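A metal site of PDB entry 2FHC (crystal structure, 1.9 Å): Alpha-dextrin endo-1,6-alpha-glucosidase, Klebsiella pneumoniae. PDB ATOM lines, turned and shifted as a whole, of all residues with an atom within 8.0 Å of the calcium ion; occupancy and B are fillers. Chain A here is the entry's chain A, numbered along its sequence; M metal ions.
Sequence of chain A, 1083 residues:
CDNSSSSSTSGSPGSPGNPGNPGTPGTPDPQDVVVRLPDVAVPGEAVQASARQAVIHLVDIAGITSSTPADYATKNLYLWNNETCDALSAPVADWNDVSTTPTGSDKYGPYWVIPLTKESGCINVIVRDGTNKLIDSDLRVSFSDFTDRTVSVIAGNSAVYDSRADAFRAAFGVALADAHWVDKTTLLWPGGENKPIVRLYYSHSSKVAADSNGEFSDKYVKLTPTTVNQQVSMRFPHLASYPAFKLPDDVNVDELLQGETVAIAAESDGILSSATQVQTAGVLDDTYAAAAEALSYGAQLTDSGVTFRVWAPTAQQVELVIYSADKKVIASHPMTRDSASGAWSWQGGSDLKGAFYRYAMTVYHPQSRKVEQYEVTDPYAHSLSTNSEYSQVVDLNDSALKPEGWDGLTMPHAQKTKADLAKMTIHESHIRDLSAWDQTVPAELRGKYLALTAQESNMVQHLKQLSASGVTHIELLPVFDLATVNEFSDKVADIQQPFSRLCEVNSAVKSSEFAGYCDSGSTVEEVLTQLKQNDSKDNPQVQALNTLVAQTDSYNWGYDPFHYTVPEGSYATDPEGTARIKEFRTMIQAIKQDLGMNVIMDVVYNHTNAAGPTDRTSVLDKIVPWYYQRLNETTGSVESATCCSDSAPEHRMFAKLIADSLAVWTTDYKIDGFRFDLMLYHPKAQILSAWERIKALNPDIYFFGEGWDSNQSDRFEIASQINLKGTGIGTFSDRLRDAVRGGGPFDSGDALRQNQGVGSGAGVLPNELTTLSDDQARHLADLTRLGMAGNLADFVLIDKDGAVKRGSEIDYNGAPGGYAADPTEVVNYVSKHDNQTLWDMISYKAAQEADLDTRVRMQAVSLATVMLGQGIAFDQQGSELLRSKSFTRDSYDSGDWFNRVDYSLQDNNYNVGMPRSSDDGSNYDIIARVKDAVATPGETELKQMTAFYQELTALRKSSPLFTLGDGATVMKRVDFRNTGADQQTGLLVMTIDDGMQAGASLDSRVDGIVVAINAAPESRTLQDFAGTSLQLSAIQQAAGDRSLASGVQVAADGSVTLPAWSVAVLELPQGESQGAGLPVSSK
The side-chain amide nitrogen (NE2) of Gln 48 sits at hydrogen-bond distance from the side-chain hydroxyl (OG1) of Thr 150. The backbone NH (N) of Ala 49 is in hydrogen-bond range of the side-chain hydroxyl (OG1) of Thr 150 (3.1 Å).
The calcium ion is bound by the side-chain carboxylate (OD2) of Asp 162 (2.3 Å), the backbone carbonyl oxygen (O) of Asp 162 (2.4 Å), the backbone carbonyl oxygen (O) of Thr 150 (2.5 Å), the side-chain carboxylate (OD1) of Asp 148 (2.5 Å) and the side-chain carboxylate (OD2) of Asp 148 (2.6 Å). The calcium ion has five donor atoms within binding distance.
Along chain A the residues within 4 Å of the calcium ion span positions 148 to 162.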
ATOM      1  N   GLU A  45     -18.881   4.213  -3.851  1.00  0.00           N
ATOM      2  CA  GLU A  45     -17.467   4.384  -3.550  1.00  0.00           C
ATOM      3  C   GLU A  45     -16.606   3.564  -4.509  1.00  0.00           C
ATOM      4  O   GLU A  45     -16.827   2.366  -4.676  1.00  0.00           O
ATOM      5  CB  GLU A  45     -17.180   3.967  -2.105  1.00  0.00           C
ATOM      6  CG  GLU A  45     -17.881   4.834  -1.074  1.00  0.00           C
ATOM      7  CD  GLU A  45     -17.478   6.293  -1.151  1.00  0.00           C
ATOM      8  OE1 GLU A  45     -16.339   6.623  -0.759  1.00  0.00           O
ATOM      9  OE2 GLU A  45     -18.297   7.103  -1.622  1.00  0.00           O
ATOM     10  N   VAL A  47     -13.355   2.922  -4.222  1.00  0.00           N
ATOM     11  CA  VAL A  47     -12.496   2.048  -3.431  1.00  0.00           C
ATOM     12  C   VAL A  47     -12.358   2.584  -2.010  1.00  0.00           C
ATOM     13  O   VAL A  47     -12.554   3.766  -1.753  1.00  0.00           O
ATOM     14  CB  VAL A  47     -11.086   1.937  -4.071  1.00  0.00           C
ATOM     15  CG1 VAL A  47     -10.386   3.289  -4.031  1.00  0.00           C
ATOM     16  CG2 VAL A  47     -10.267   0.888  -3.351  1.00  0.00           C
ATOM     17  N   GLN A  48     -12.019   1.689  -1.085  1.00  0.00           N
ATOM     18  CA  GLN A  48     -11.832   2.060   0.325  1.00  0.00           C
ATOM     19  C   GLN A  48     -10.366   1.917   0.708  1.00  0.00           C
ATOM     20  O   GLN A  48      -9.746   0.887   0.442  1.00  0.00           O
ATOM     21  CB  GLN A  48     -12.697   1.168   1.224  1.00  0.00           C
ATOM     22  CG  GLN A  48     -14.198   1.415   1.082  1.00  0.00           C
ATOM     23  CD  GLN A  48     -14.640   2.751   1.654  1.00  0.00           C
ATOM     24  OE1 GLN A  48     -15.786   3.160   1.490  1.00  0.00           O
ATOM     25  NE2 GLN A  48     -13.729   3.440   2.332  1.00  0.00           N
ATOM     26  N   ALA A  49      -9.819   2.955   1.329  1.00  0.00           N
ATOM     27  CA  ALA A  49      -8.415   2.947   1.741  1.00  0.00           C
ATOM     28  C   ALA A  49      -8.076   1.711   2.561  1.00  0.00           C
ATOM     29  O   ALA A  49      -8.864   1.272   3.405  1.00  0.00           O
ATOM     30  CB  ALA A  49      -8.111   4.208   2.544  1.00  0.00           C
ATOM     31  N   VAL A  55      -7.573   7.306   0.419  1.00  0.00           N
ATOM     32  CA  VAL A  55      -7.989   7.517  -0.962  1.00  0.00           C
ATOM     33  C   VAL A  55      -8.864   8.762  -1.093  1.00  0.00           C
ATOM     34  O   VAL A  55      -9.721   9.023  -0.249  1.00  0.00           O
ATOM     35  CB  VAL A  55      -8.774   6.302  -1.503  1.00  0.00           C
ATOM     36  CG1 VAL A  55      -7.883   5.061  -1.492  1.00  0.00           C
ATOM     37  CG2 VAL A  55     -10.028   6.068  -0.686  1.00  0.00           C
ATOM     38  N   HIS A  57     -11.388  10.809  -3.753  1.00  0.00           N
ATOM     39  CA  HIS A  57     -12.183  10.763  -4.972  1.00  0.00           C
ATOM     40  C   HIS A  57     -12.444  12.173  -5.482  1.00  0.00           C
ATOM     41  O   HIS A  57     -12.534  13.118  -4.706  1.00  0.00           O
ATOM     42  CB  HIS A  57     -13.532  10.084  -4.705  1.00  0.00           C
ATOM     43  CG  HIS A  57     -13.422   8.689  -4.166  1.00  0.00           C
ATOM     44  ND1 HIS A  57     -12.930   7.642  -4.913  1.00  0.00           N
ATOM     45  CD2 HIS A  57     -13.742   8.176  -2.959  1.00  0.00           C
ATOM     46  CE1 HIS A  57     -12.968   6.539  -4.183  1.00  0.00           C
ATOM     47  NE2 HIS A  57     -13.458   6.841  -2.993  1.00  0.00           N
ATOM     48  N   ASP A 145     -12.105  12.992  11.785  1.00  0.00           N
ATOM     49  CA  ASP A 145     -13.458  13.244  11.310  1.00  0.00           C
ATOM     50  C   ASP A 145     -13.878  12.168  10.310  1.00  0.00           C
ATOM     51  O   ASP A 145     -15.056  11.803  10.234  1.00  0.00           O
ATOM     52  CB  ASP A 145     -13.553  14.621  10.651  1.00  0.00           C
ATOM     53  CG  ASP A 145     -13.258  15.751  11.623  1.00  0.00           C
ATOM     54  OD1 ASP A 145     -12.129  15.783  12.178  1.00  0.00           O
ATOM     55  OD2 ASP A 145     -14.139  16.603  11.843  1.00  0.00           O
ATOM     56  N   PHE A 146     -12.913  11.670   9.546  1.00  0.00           N
ATOM     57  CA  PHE A 146     -13.161  10.627   8.555  1.00  0.00           C
ATOM     58  C   PHE A 146     -12.260   9.445   8.867  1.00  0.00           C
ATOM     59  O   PHE A 146     -11.198   9.283   8.271  1.00  0.00           O
ATOM     60  CB  PHE A 146     -12.880  11.154   7.149  1.00  0.00           C
ATOM     61  CG  PHE A 146     -13.592  12.434   6.825  1.00  0.00           C
ATOM     62  CD1 PHE A 146     -13.092  13.657   7.266  1.00  0.00           C
ATOM     63  CD2 PHE A 146     -14.770  12.425   6.097  1.00  0.00           C
ATOM     64  CE1 PHE A 146     -13.753  14.843   6.988  1.00  0.00           C
ATOM     65  CE2 PHE A 146     -15.451  13.608   5.806  1.00  0.00           C
ATOM     66  CZ  PHE A 146     -14.942  14.826   6.256  1.00  0.00           C
ATOM     67  N   THR A 147     -12.700   8.616   9.802  1.00  0.00           N
ATOM     68  CA  THR A 147     -11.946   7.439  10.227  1.00  0.00           C
ATOM     69  C   THR A 147     -11.484   6.524   9.094  1.00  0.00           C
ATOM     70  O   THR A 147     -10.341   6.086   9.074  1.00  0.00           O
ATOM     71  CB  THR A 147     -12.753   6.596  11.246  1.00  0.00           C
ATOM     72  OG1 THR A 147     -11.994   5.455  11.645  1.00  0.00           O
ATOM     73  CG2 THR A 147     -14.070   6.143  10.629  1.00  0.00           C
ATOM     74  N   ASP A 148     -12.380   6.246   8.142  1.00  0.00           N
ATOM     75  CA  ASP A 148     -12.038   5.362   7.025  1.00  0.00           C
ATOM     76  C   ASP A 148     -11.001   5.972   6.088  1.00  0.00           C
ATOM     77  O   ASP A 148     -10.541   5.315   5.154  1.00  0.00           O
ATOM     78  CB  ASP A 148     -13.299   5.005   6.237  1.00  0.00           C
ATOM     79  CG  ASP A 148     -14.037   6.217   5.719  1.00  0.00           C
ATOM     80  OD1 ASP A 148     -13.437   7.019   4.976  1.00  0.00           O
ATOM     81  OD2 ASP A 148     -15.237   6.374   6.053  1.00  0.00           O
ATOM     82  N   ARG A 149     -10.640   7.230   6.343  1.00  0.00           N
ATOM     83  CA  ARG A 149      -9.652   7.937   5.529  1.00  0.00           C
ATOM     84  C   ARG A 149      -9.990   7.910   4.034  1.00  0.00           C
ATOM     85  O   ARG A 149      -9.098   7.987   3.184  1.00  0.00           O
ATOM     86  CB  ARG A 149      -8.252   7.338   5.754  1.00  0.00           C
ATOM     87  CG  ARG A 149      -7.780   7.387   7.193  1.00  0.00           C
ATOM     88  CD  ARG A 149      -6.335   6.908   7.314  1.00  0.00           C
ATOM     89  NE  ARG A 149      -6.136   5.567   6.773  1.00  0.00           N
ATOM     90  CZ  ARG A 149      -6.733   4.476   7.246  1.00  0.00           C
ATOM     91  NH1 ARG A 149      -7.562   4.553   8.270  1.00  0.00           N
ATOM     92  NH2 ARG A 149      -6.491   3.293   6.678  1.00  0.00           N
ATOM     93  N   THR A 150     -11.278   7.810   3.734  1.00  0.00           N
ATOM     94  CA  THR A 150     -11.742   7.777   2.349  1.00  0.00           C
ATOM     95  C   THR A 150     -12.708   8.950   2.128  1.00  0.00           C
ATOM     96  O   THR A 150     -13.859   8.895   2.561  1.00  0.00           O
ATOM     97  CB  THR A 150     -12.477   6.454   2.039  1.00  0.00           C
ATOM     98  OG1 THR A 150     -11.573   5.358   2.204  1.00  0.00           O
ATOM     99  CG2 THR A 150     -13.007   6.458   0.610  1.00  0.00           C
ATOM    100  N   VAL A 151     -12.225   9.984   1.447  1.00  0.00           N
ATOM    101  CA  VAL A 151     -13.048  11.168   1.189  1.00  0.00           C
ATOM    102  C   VAL A 151     -13.180  11.493  -0.289  1.00  0.00           C
ATOM    103  O   VAL A 151     -12.454  10.964  -1.124  1.00  0.00           O
ATOM    104  CB  VAL A 151     -12.461  12.400   1.912  1.00  0.00           C
ATOM    105  CG1 VAL A 151     -12.416  12.153   3.422  1.00  0.00           C
ATOM    106  CG2 VAL A 151     -11.076  12.707   1.380  1.00  0.00           C
ATOM    107  N   SER A 152     -14.122  12.386  -0.605  1.00  0.00           N
ATOM    108  CA  SER A 152     -14.372  12.809  -1.976  1.00  0.00           C
ATOM    109  C   SER A 152     -14.527  14.328  -2.051  1.00  0.00           C
ATOM    110  O   SER A 152     -15.168  14.931  -1.193  1.00  0.00           O
ATOM    111  CB  SER A 152     -15.640  12.132  -2.511  1.00  0.00           C
ATOM    112  OG  SER A 152     -15.525  10.724  -2.496  1.00  0.00           O
ATOM    113  N   TYR A 161     -15.918  15.592   1.889  1.00  0.00           N
ATOM    114  CA  TYR A 161     -17.034  14.698   2.180  1.00  0.00           C
ATOM    115  C   TYR A 161     -16.539  13.291   2.443  1.00  0.00           C
ATOM    116  O   TYR A 161     -15.469  12.899   1.967  1.00  0.00           O
ATOM    117  CB  TYR A 161     -18.027  14.716   1.010  1.00  0.00           C
ATOM    118  CG  TYR A 161     -18.659  16.074   0.812  1.00  0.00           C
ATOM    119  CD1 TYR A 161     -19.542  16.600   1.755  1.00  0.00           C
ATOM    120  CD2 TYR A 161     -18.375  16.831  -0.320  1.00  0.00           C
ATOM    121  CE1 TYR A 161     -20.103  17.859   1.591  1.00  0.00           C
ATOM    122  CE2 TYR A 161     -18.935  18.099  -0.502  1.00  0.00           C
ATOM    123  CZ  TYR A 161     -19.800  18.601   0.465  1.00  0.00           C
ATOM    124  OH  TYR A 161     -20.361  19.850   0.296  1.00  0.00           O
ATOM    125  N   ASP A 162     -17.317  12.525   3.200  1.00  0.00           N
ATOM    126  CA  ASP A 162     -16.943  11.162   3.542  1.00  0.00           C
ATOM    127  C   ASP A 162     -17.353  10.167   2.449  1.00  0.00           C
ATOM    128  O   ASP A 162     -17.221   8.958   2.622  1.00  0.00           O
ATOM    129  CB  ASP A 162     -17.583  10.756   4.877  1.00  0.00           C
ATOM    130  CG  ASP A 162     -16.764   9.715   5.624  1.00  0.00           C
ATOM    131  OD1 ASP A 162     -17.224   9.258   6.690  1.00  0.00           O
ATOM    132  OD2 ASP A 162     -15.662   9.365   5.150  1.00  0.00           O
ATOM    133  N   SER A 163     -17.840  10.685   1.330  1.00  0.00           N
ATOM    134  CA  SER A 163     -18.259   9.835   0.219  1.00  0.00           C
ATOM    135  C   SER A 163     -18.576  10.651  -1.037  1.00  0.00           C
ATOM    136  O   SER A 163     -18.863  11.842  -0.963  1.00  0.00           O
ATOM    137  CB  SER A 163     -19.494   9.025   0.621  1.00  0.00           C
ATOM    138  OG  SER A 163     -20.598   9.880   0.879  1.00  0.00           O
ATOM    139  N   ARG A 164     -18.526   9.991  -2.189  1.00  0.00           N
ATOM    140  CA  ARG A 164     -18.835  10.654  -3.455  1.00  0.00           C
ATOM    141  C   ARG A 164     -20.328  10.944  -3.484  1.00  0.00           C
ATOM    142  O   ARG A 164     -20.789  11.806  -4.223  1.00  0.00           O
ATOM    143  CB  ARG A 164     -18.439   9.758  -4.640  1.00  0.00           C
ATOM    144  CG  ARG A 164     -16.954   9.430  -4.709  1.00  0.00           C
ATOM    145  CD  ARG A 164     -16.541   8.911  -6.084  1.00  0.00           C
ATOM    146  NE  ARG A 164     -17.124   7.608  -6.404  1.00  0.00           N
ATOM    147  CZ  ARG A 164     -16.867   6.927  -7.515  1.00  0.00           C
ATOM    148  NH1 ARG A 164     -16.040   7.432  -8.423  1.00  0.00           N
ATOM    149  NH2 ARG A 164     -17.436   5.747  -7.726  1.00  0.00           N
ATOM    150  N   ASP A 166     -22.168  12.112  -0.938  1.00  0.00           N
ATOM    151  CA  ASP A 166     -22.407  13.397  -0.284  1.00  0.00           C
ATOM    152  C   ASP A 166     -22.004  14.551  -1.192  1.00  0.00           C
ATOM    153  O   ASP A 166     -22.727  15.534  -1.330  1.00  0.00           O
ATOM    154  CB  ASP A 166     -21.623  13.487   1.024  1.00  0.00           C
ATOM    155  CG  ASP A 166     -22.196  12.590   2.104  1.00  0.00           C
ATOM    156  OD1 ASP A 166     -21.576  12.489   3.188  1.00  0.00           O
ATOM    157  OD2 ASP A 166     -23.263  11.994   1.876  1.00  0.00           O
HETATM  158 CA    CA M   1     -15.585   7.557   3.754  1.00  0.00          CA
